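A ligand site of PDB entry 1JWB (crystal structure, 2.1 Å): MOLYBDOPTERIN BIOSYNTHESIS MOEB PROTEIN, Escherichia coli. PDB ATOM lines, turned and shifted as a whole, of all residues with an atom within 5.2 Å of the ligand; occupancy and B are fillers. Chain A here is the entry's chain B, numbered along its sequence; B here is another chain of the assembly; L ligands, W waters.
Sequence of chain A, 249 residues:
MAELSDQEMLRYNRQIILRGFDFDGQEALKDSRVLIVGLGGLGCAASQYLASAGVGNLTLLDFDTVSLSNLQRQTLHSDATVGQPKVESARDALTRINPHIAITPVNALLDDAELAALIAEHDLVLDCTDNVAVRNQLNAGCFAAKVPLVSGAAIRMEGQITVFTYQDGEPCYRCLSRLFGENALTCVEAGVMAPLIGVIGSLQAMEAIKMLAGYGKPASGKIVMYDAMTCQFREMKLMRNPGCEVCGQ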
ATOM      1  N   VAL A  37       0.116  10.724   7.288  1.00  0.00           N
ATOM      2  CA  VAL A  37       1.050  10.468   6.186  1.00  0.00           C
ATOM      3  C   VAL A  37       0.625   9.213   5.421  1.00  0.00           C
ATOM      4  O   VAL A  37       0.657   8.120   5.949  1.00  0.00           O
ATOM      5  CB  VAL A  37       2.499  10.288   6.705  1.00  0.00           C
ATOM      6  CG1 VAL A  37       3.463  10.283   5.541  1.00  0.00           C
ATOM      7  CG2 VAL A  37       2.864  11.412   7.651  1.00  0.00           C
ATOM      8  N   GLY A  38       0.210   9.421   4.162  1.00  0.00           N
ATOM      9  CA  GLY A  38      -0.356   8.377   3.322  1.00  0.00           C
ATOM     10  C   GLY A  38      -1.896   8.437   3.287  1.00  0.00           C
ATOM     11  O   GLY A  38      -2.589   8.121   4.273  1.00  0.00           O
ATOM     12  N   LEU A  39      -2.446   8.888   2.181  1.00  0.00           N
ATOM     13  CA  LEU A  39      -3.876   8.975   2.026  1.00  0.00           C
ATOM     14  C   LEU A  39      -4.266   7.946   1.006  1.00  0.00           C
ATOM     15  O   LEU A  39      -5.006   8.208   0.038  1.00  0.00           O
ATOM     16  CB  LEU A  39      -4.320  10.383   1.638  1.00  0.00           C
ATOM     17  CG  LEU A  39      -4.623  11.282   2.819  1.00  0.00           C
ATOM     18  CD1 LEU A  39      -5.798  10.745   3.633  1.00  0.00           C
ATOM     19  CD2 LEU A  39      -3.403  11.483   3.698  1.00  0.00           C
ATOM     20  N   GLY A  40      -3.723   6.758   1.251  1.00  0.00           N
ATOM     21  CA  GLY A  40      -4.047   5.594   0.481  1.00  0.00           C
ATOM     22  C   GLY A  40      -5.107   4.858   1.275  1.00  0.00           C
ATOM     23  O   GLY A  40      -5.954   5.447   1.921  1.00  0.00           O
ATOM     24  N   GLY A  41      -4.989   3.551   1.325  1.00  0.00           N
ATOM     25  CA  GLY A  41      -5.940   2.719   2.036  1.00  0.00           C
ATOM     26  C   GLY A  41      -6.040   3.016   3.506  1.00  0.00           C
ATOM     27  O   GLY A  41      -7.137   3.305   4.042  1.00  0.00           O
ATOM     28  N   LEU A  42      -4.909   2.943   4.190  1.00  0.00           N
ATOM     29  CA  LEU A  42      -4.955   3.264   5.623  1.00  0.00           C
ATOM     30  C   LEU A  42      -5.413   4.689   5.884  1.00  0.00           C
ATOM     31  O   LEU A  42      -6.228   4.960   6.782  1.00  0.00           O
ATOM     32  CB  LEU A  42      -3.604   3.005   6.309  1.00  0.00           C
ATOM     33  CG  LEU A  42      -3.303   1.510   6.423  1.00  0.00           C
ATOM     34  CD1 LEU A  42      -1.903   1.286   7.010  1.00  0.00           C
ATOM     35  CD2 LEU A  42      -4.351   0.769   7.238  1.00  0.00           C
ATOM     36  N   LEU A  61      -0.754  14.303   3.962  1.00  0.00           N
ATOM     37  CA  LEU A  61       0.493  14.310   3.256  1.00  0.00           C
ATOM     38  C   LEU A  61       0.655  13.064   2.437  1.00  0.00           C
ATOM     39  O   LEU A  61       0.687  11.934   2.971  1.00  0.00           O
ATOM     40  CB  LEU A  61       1.652  14.417   4.256  1.00  0.00           C
ATOM     41  CG  LEU A  61       3.038  14.314   3.632  1.00  0.00           C
ATOM     42  CD1 LEU A  61       3.280  15.476   2.685  1.00  0.00           C
ATOM     43  CD2 LEU A  61       4.120  14.299   4.722  1.00  0.00           C
ATOM     44  N   ASP A  62       0.802  13.255   1.145  1.00  0.00           N
ATOM     45  CA  ASP A  62       0.983  12.185   0.193  1.00  0.00           C
ATOM     46  C   ASP A  62       1.495  12.874  -1.081  1.00  0.00           C
ATOM     47  O   ASP A  62       1.139  14.040  -1.364  1.00  0.00           O
ATOM     48  CB  ASP A  62      -0.307  11.435  -0.070  1.00  0.00           C
ATOM     49  CG  ASP A  62      -0.077  10.019  -0.557  1.00  0.00           C
ATOM     50  OD1 ASP A  62       0.799   9.820  -1.425  1.00  0.00           O
ATOM     51  OD2 ASP A  62      -0.775   9.041  -0.150  1.00  0.00           O
ATOM     52  N   PHE A  63       2.298  12.141  -1.840  1.00  0.00           N
ATOM     53  CA  PHE A  63       2.889  12.692  -3.060  1.00  0.00           C
ATOM     54  C   PHE A  63       2.190  12.124  -4.269  1.00  0.00           C
ATOM     55  O   PHE A  63       2.399  12.565  -5.403  1.00  0.00           O
ATOM     56  CB  PHE A  63       4.356  12.280  -3.165  1.00  0.00           C
ATOM     57  CG  PHE A  63       4.536  10.850  -3.343  1.00  0.00           C
ATOM     58  CD1 PHE A  63       4.446  10.285  -4.581  1.00  0.00           C
ATOM     59  CD2 PHE A  63       4.712  10.025  -2.243  1.00  0.00           C
ATOM     60  CE1 PHE A  63       4.590   8.948  -4.752  1.00  0.00           C
ATOM     61  CE2 PHE A  63       4.828   8.691  -2.396  1.00  0.00           C
ATOM     62  CZ  PHE A  63       4.751   8.141  -3.658  1.00  0.00           C
ATOM     63  N   ASP A  64       1.323  11.159  -4.039  1.00  0.00           N
ATOM     64  CA  ASP A  64       0.802  10.376  -5.135  1.00  0.00           C
ATOM     65  C   ASP A  64      -0.618  10.764  -5.572  1.00  0.00           C
ATOM     66  O   ASP A  64      -1.376  11.449  -4.844  1.00  0.00           O
ATOM     67  CB  ASP A  64       0.924   8.910  -4.694  1.00  0.00           C
ATOM     68  CG  ASP A  64       0.671   7.891  -5.802  1.00  0.00           C
ATOM     69  OD1 ASP A  64       0.932   8.204  -6.976  1.00  0.00           O
ATOM     70  OD2 ASP A  64       0.243   6.739  -5.539  1.00  0.00           O
ATOM     71  N   ARG A  73     -10.116   0.028  -2.509  1.00  0.00           N
ATOM     72  CA  ARG A  73     -10.096   0.210  -1.050  1.00  0.00           C
ATOM     73  C   ARG A  73      -9.994   1.643  -0.500  1.00  0.00           C
ATOM     74  O   ARG A  73     -10.354   1.876   0.641  1.00  0.00           O
ATOM     75  CB  ARG A  73      -8.954  -0.612  -0.429  1.00  0.00           C
ATOM     76  CG  ARG A  73      -7.597  -0.106  -0.808  1.00  0.00           C
ATOM     77  CD  ARG A  73      -6.505  -1.032  -0.507  1.00  0.00           C
ATOM     78  NE  ARG A  73      -5.224  -0.433  -0.834  1.00  0.00           N
ATOM     79  CZ  ARG A  73      -4.706  -0.367  -2.026  1.00  0.00           C
ATOM     80  NH1 ARG A  73      -5.333  -0.863  -3.069  1.00  0.00           N
ATOM     81  NH2 ARG A  73      -3.552   0.229  -2.177  1.00  0.00           N
ATOM     82  N   GLN A  74      -9.566   2.603  -1.291  1.00  0.00           N
ATOM     83  CA  GLN A  74      -9.408   3.954  -0.792  1.00  0.00           C
ATOM     84  C   GLN A  74     -10.671   4.734  -1.029  1.00  0.00           C
ATOM     85  O   GLN A  74     -10.762   5.534  -1.971  1.00  0.00           O
ATOM     86  CB  GLN A  74      -8.205   4.530  -1.515  1.00  0.00           C
ATOM     87  CG  GLN A  74      -6.989   3.620  -1.376  1.00  0.00           C
ATOM     88  CD  GLN A  74      -5.787   4.066  -2.147  1.00  0.00           C
ATOM     89  OE1 GLN A  74      -4.831   3.319  -2.251  1.00  0.00           O
ATOM     90  NE2 GLN A  74      -5.814   5.260  -2.682  1.00  0.00           N
ATOM     91  N   LYS A  86      -3.848  12.418  -4.268  1.00  0.00           N
ATOM     92  CA  LYS A  86      -4.659  11.823  -3.213  1.00  0.00           C
ATOM     93  C   LYS A  86      -5.066  12.786  -2.095  1.00  0.00           C
ATOM     94  O   LYS A  86      -6.192  12.724  -1.557  1.00  0.00           O
ATOM     95  CB  LYS A  86      -3.917  10.627  -2.617  1.00  0.00           C
ATOM     96  CG  LYS A  86      -3.820   9.472  -3.579  1.00  0.00           C
ATOM     97  CD  LYS A  86      -3.016   8.342  -2.959  1.00  0.00           C
ATOM     98  CE  LYS A  86      -3.023   7.115  -3.840  1.00  0.00           C
ATOM     99  NZ  LYS A  86      -1.934   6.202  -3.524  1.00  0.00           N
ATOM    100  N   ALA A 108       3.202  16.331  -1.575  1.00  0.00           N
ATOM    101  CA  ALA A 108       4.622  16.419  -1.758  1.00  0.00           C
ATOM    102  C   ALA A 108       5.229  15.202  -1.196  1.00  0.00           C
ATOM    103  O   ALA A 108       4.587  14.467  -0.480  1.00  0.00           O
ATOM    104  CB  ALA A 108       5.166  17.651  -1.028  1.00  0.00           C
ATOM    105  N   LEU A 109       6.493  15.002  -1.548  1.00  0.00           N
ATOM    106  CA  LEU A 109       7.299  13.997  -0.942  1.00  0.00           C
ATOM    107  C   LEU A 109       8.300  14.795  -0.151  1.00  0.00           C
ATOM    108  O   LEU A 109       9.180  15.430  -0.722  1.00  0.00           O
ATOM    109  CB  LEU A 109       7.961  13.162  -2.014  1.00  0.00           C
ATOM    110  CG  LEU A 109       8.924  12.155  -1.442  1.00  0.00           C
ATOM    111  CD1 LEU A 109       8.228  11.109  -0.724  1.00  0.00           C
ATOM    112  CD2 LEU A 109       9.677  11.562  -2.597  1.00  0.00           C
ATOM    113  N   LEU A 110       8.217  14.747   1.178  1.00  0.00           N
ATOM    114  CA  LEU A 110       9.065  15.602   1.970  1.00  0.00           C
ATOM    115  C   LEU A 110      10.392  14.990   2.315  1.00  0.00           C
ATOM    116  O   LEU A 110      10.552  13.760   2.388  1.00  0.00           O
ATOM    117  CB  LEU A 110       8.358  15.977   3.267  1.00  0.00           C
ATOM    118  CG  LEU A 110       6.997  16.663   3.052  1.00  0.00           C
ATOM    119  CD1 LEU A 110       6.389  17.071   4.339  1.00  0.00           C
ATOM    120  CD2 LEU A 110       7.121  17.888   2.214  1.00  0.00           C
ATOM    121  N   CYS A 128       0.509   6.129   7.731  1.00  0.00           N
ATOM    122  CA  CYS A 128      -0.334   5.302   6.889  1.00  0.00           C
ATOM    123  C   CYS A 128       0.344   5.105   5.553  1.00  0.00           C
ATOM    124  O   CYS A 128      -0.301   5.078   4.559  1.00  0.00           O
ATOM    125  CB  CYS A 128      -1.683   5.973   6.662  1.00  0.00           C
ATOM    126  SG  CYS A 128      -2.639   6.365   8.148  1.00  0.00           S
ATOM    127  N   THR A 129       1.638   4.887   5.582  1.00  0.00           N
ATOM    128  CA  THR A 129       2.433   4.741   4.399  1.00  0.00           C
ATOM    129  C   THR A 129       2.577   3.279   3.988  1.00  0.00           C
ATOM    130  O   THR A 129       1.922   2.412   4.575  1.00  0.00           O
ATOM    131  CB  THR A 129       3.817   5.356   4.677  1.00  0.00           C
ATOM    132  OG1 THR A 129       4.428   4.618   5.734  1.00  0.00           O
ATOM    133  CG2 THR A 129       3.648   6.705   5.246  1.00  0.00           C
ATOM    134  N   ASP A 130       3.431   3.004   3.021  1.00  0.00           N
ATOM    135  CA  ASP A 130       3.544   1.664   2.513  1.00  0.00           C
ATOM    136  C   ASP A 130       4.950   1.245   2.282  1.00  0.00           C
ATOM    137  O   ASP A 130       5.217   0.468   1.456  1.00  0.00           O
ATOM    138  CB  ASP A 130       2.772   1.569   1.192  1.00  0.00           C
ATOM    139  CG  ASP A 130       3.216   2.618   0.168  1.00  0.00           C
ATOM    140  OD1 ASP A 130       4.233   3.318   0.421  1.00  0.00           O
ATOM    141  OD2 ASP A 130       2.571   2.861  -0.884  1.00  0.00           O
ATOM    142  N   ASN A 131       5.875   1.806   3.009  1.00  0.00           N
ATOM    143  CA  ASN A 131       7.280   1.467   2.830  1.00  0.00           C
ATOM    144  C   ASN A 131       8.066   1.830   4.084  1.00  0.00           C
ATOM    145  O   ASN A 131       7.814   2.824   4.755  1.00  0.00           O
ATOM    146  CB  ASN A 131       7.880   2.110   1.559  1.00  0.00           C
ATOM    147  CG  ASN A 131       7.943   3.622   1.622  1.00  0.00           C
ATOM    148  OD1 ASN A 131       8.929   4.197   2.122  1.00  0.00           O
ATOM    149  ND2 ASN A 131       6.918   4.294   1.085  1.00  0.00           N
ATOM    150  N   VAL A 134       9.910   5.525   4.624  1.00  0.00           N
ATOM    151  CA  VAL A 134       9.238   6.685   5.176  1.00  0.00           C
ATOM    152  C   VAL A 134       8.804   6.359   6.608  1.00  0.00           C
ATOM    153  O   VAL A 134       8.833   7.199   7.478  1.00  0.00           O
ATOM    154  CB  VAL A 134       8.072   7.238   4.288  1.00  0.00           C
ATOM    155  CG1 VAL A 134       6.989   6.258   4.195  1.00  0.00           C
ATOM    156  CG2 VAL A 134       7.504   8.503   4.837  1.00  0.00           C
ATOM    157  N   GLN A 137      11.658   7.231   8.657  1.00  0.00           N
ATOM    158  CA  GLN A 137      11.768   8.672   8.697  1.00  0.00           C
ATOM    159  C   GLN A 137      10.772   9.254   9.680  1.00  0.00           C
ATOM    160  O   GLN A 137      11.057  10.171  10.455  1.00  0.00           O
ATOM    161  CB  GLN A 137      11.395   9.302   7.340  1.00  0.00           C
ATOM    162  CG  GLN A 137      12.537   9.687   6.462  1.00  0.00           C
ATOM    163  CD  GLN A 137      12.022  10.363   5.210  1.00  0.00           C
ATOM    164  OE1 GLN A 137      11.011   9.941   4.642  1.00  0.00           O
ATOM    165  NE2 GLN A 137      12.685  11.428   4.802  1.00  0.00           N
ATOM    166  N   GLY B  80       3.145  -2.535   4.311  1.00  0.00           N
ATOM    167  CA  GLY B  80       2.266  -1.895   3.365  1.00  0.00           C
ATOM    168  C   GLY B  80       1.199  -1.094   4.080  1.00  0.00           C
ATOM    169  O   GLY B  80       1.044  -1.188   5.261  1.00  0.00           O
ATOM    170  N   GLY B  81       0.407  -0.348   3.339  1.00  0.00           N
ATOM    171  CA  GLY B  81      -0.682   0.351   3.938  1.00  0.00           C
ATOM    172  C   GLY B  81      -1.297   1.229   2.919  1.00  0.00           C
ATOM    173  O   GLY B  81      -2.220   2.006   3.178  1.00  0.00           O
HETATM  174  P1  LIG L   1      -1.340   2.353   0.406  1.00  0.00           P
HETATM  175  O1  LIG L   1      -0.771   1.465   1.397  1.00  0.00           O
HETATM  176  O2  LIG L   1      -0.497   2.157  -0.845  1.00  0.00           O
HETATM  177  O3  LIG L   1      -2.829   1.970   0.308  1.00  0.00           O
HETATM  178  O4  LIG L   1      -1.162   3.791   1.072  1.00  0.00           O
HETATM  179  C1  LIG L   1       0.100   4.305   1.400  1.00  0.00           C
HETATM  180  C2  LIG L   1       0.089   5.739   0.942  1.00  0.00           C
HETATM  181  O5  LIG L   1       1.275   6.203   1.457  1.00  0.00           O
HETATM  182  C3  LIG L   1       0.148   6.026  -0.542  1.00  0.00           C
HETATM  183  O6  LIG L   1      -1.003   6.625  -0.975  1.00  0.00           O
HETATM  184  C4  LIG L   1       1.568   6.441  -0.832  1.00  0.00           C
HETATM  185  O7  LIG L   1       1.575   7.374  -1.909  1.00  0.00           O
HETATM  186  C5  LIG L   1       1.866   7.046   0.519  1.00  0.00           C
HETATM  187  N1  LIG L   1       3.290   7.280   0.771  1.00  0.00           N
HETATM  188  C6  LIG L   1       4.319   6.415   0.689  1.00  0.00           C
HETATM  189  N2  LIG L   1       5.455   7.080   0.981  1.00  0.00           N
HETATM  190  C7  LIG L   1       5.137   8.380   1.231  1.00  0.00           C
HETATM  191  C8  LIG L   1       5.918   9.484   1.544  1.00  0.00           C
HETATM  192  N3  LIG L   1       7.229   9.368   1.648  1.00  0.00           N
HETATM  193  N4  LIG L   1       5.270  10.675   1.755  1.00  0.00           N
HETATM  194  C9  LIG L   1       3.877  10.774   1.623  1.00  0.00           C
HETATM  195  N5  LIG L   1       3.131   9.667   1.279  1.00  0.00           N
HETATM  196  C10 LIG L   1       3.777   8.499   1.115  1.00  0.00           C
HETATM  197  O   HOH W   1      -1.837   3.366  -3.021  1.00  0.00           O
HETATM  198  O   HOH W   2      -2.625   5.195   3.323  1.00  0.00           O
HETATM  199  O   HOH W   3       0.950   3.240  -3.297  1.00  0.00           O
HETATM  200  O   HOH W   4       9.112   7.161   1.192  1.00  0.00           O
HETATM  201  O   HOH W   5       2.223   5.459  -3.815  1.00  0.00           O
HETATM  202  O   HOH W   6      -3.882  -0.122   1.425  1.00  0.00           O
HETATM  203  O   HOH W   7       6.199  13.268   2.180  1.00  0.00           O
HETATM  204  O   HOH W   8       0.609  -1.206   0.267  1.00  0.00           O
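Val 37 touches the ligand (CG1 to C9, 3.97 Å).
CA of Gly 38 touches O5 of the ligand, 3.3 Å away.
CA of Gly 40 touches O4 of the ligand, 3.5 Å away.
Leu 61 touches the ligand (O to C9, 3.7 Å).
Phe 63 touches the ligand (CE2 to O7, 3.5 Å).
Asp 64 touches the ligand.
Gln 74 touches the ligand (OE1 to O3, 3.5 Å).
Leu 109 touches the ligand.
O of Cys 128 touches C1 of the ligand, 3.3 Å away.
Thr 129 touches the ligand.
CG2 of Val 134 touches N3 of the ligand, 3.3 Å away.
Hydrophobic or aromatic side chains that line the ligand: Val 37, Phe 63, Leu 109 and Val 134.
18 residues have an atom within 4 Å of the ligand: Val 37, Gly 38, Gly 40, Gly 41, Leu 61, Asp 62, Phe 63, Asp 64, Arg 73, Gln 74, Lys 86, Leu 109, Cys 128, Thr 129, Asp 130, Asn 131, Val 134 and Gly 81 of chain B.
The nearest printed residue that does not touch the ligand is Leu 39 (4.04 Å).
O of Thr 129 lies close to N of Gly 81 of chain B, at 3.4 Å.
The backbone NH of Asp 64 sits at hydrogen-bond distance from the side-chain carboxylate of Asp 62 (3.0 Å).
OD2 of Asp 64 is in salt-bridge range of NZ of Lys 86 (3.0 Å).
ND2 of Asn 131 sits at hydrogen-bond distance from OD1 of Asp 130, at 2.9 Å.
NH2 of Arg 73 lies within hydrogen-bond range of OE1 of Gln 74 (3.3 Å).
The backbone NH (N) of Val 134 sits at hydrogen-bond distance from the side-chain amide oxygen (OD1) of Asn 131.
The backbone carbonyl oxygen (O) of Val 37 is in hydrogen-bond range of the backbone NH (N) of Cys 128 (2.7 Å).
N of Gly 38 lies within hydrogen-bond range of O of Leu 61 (2.8 Å).
Water W6 lies within hydrogen-bond range of O3 of the ligand (2.6 Å), NE of Arg 73 (2.6 Å) and O of Gly 81 of chain B (3.2 Å).
Water W5 lies within hydrogen-bond range of an oxygen (O7) of the ligand (2.8 Å) and the side-chain carboxylate (OD2) of Asp 64 (2.9 Å).
Water W1 lies within hydrogen-bond range of O2 of the ligand, NZ of Lys 86 and OE1 of Gln 74.
Water W4 lies within hydrogen-bond range of a nitrogen (N3) of the ligand (2.9 Å) and the side-chain amide oxygen (OD1) of Asn 131 (3.1 Å).
Water W3 bridges OD2 of Asp 130 (2.9 Å) and O2 of the ligand (3.0 Å).
Water W8 lies within hydrogen-bond range of the backbone NH of Gly 81 of chain B (3.2 Å) and an oxygen (O1) of the ligand (3.2 Å).
N of Gly 81 of chain B lies close to O1 of the ligand (2.9 Å).
O of Gly 81 of chain B sits at hydrogen-bond distance from O3 of the ligand (2.9 Å).
The side-chain carboxylate (OD2) of Asp 62 is in hydrogen-bond range of an oxygen (O6) of the ligand, 2.6 Å away.
NZ of Lys 86 lies within hydrogen-bond range of O6 of the ligand, at 2.7 Å.
N of Gly 41 is in hydrogen-bond range of O3 of the ligand (2.9 Å).
The side-chain carboxylate (OD2) of Asp 130 lies within hydrogen-bond range of an oxygen (O2) of the ligand (3.1 Å).
The guanidinium group of Arg 73 lies within hydrogen-bond range of an oxygen (O3) of the ligand (3.1 Å).
ND2 of Asn 131 sits at hydrogen-bond distance from N2 of the ligand (3.1 Å).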
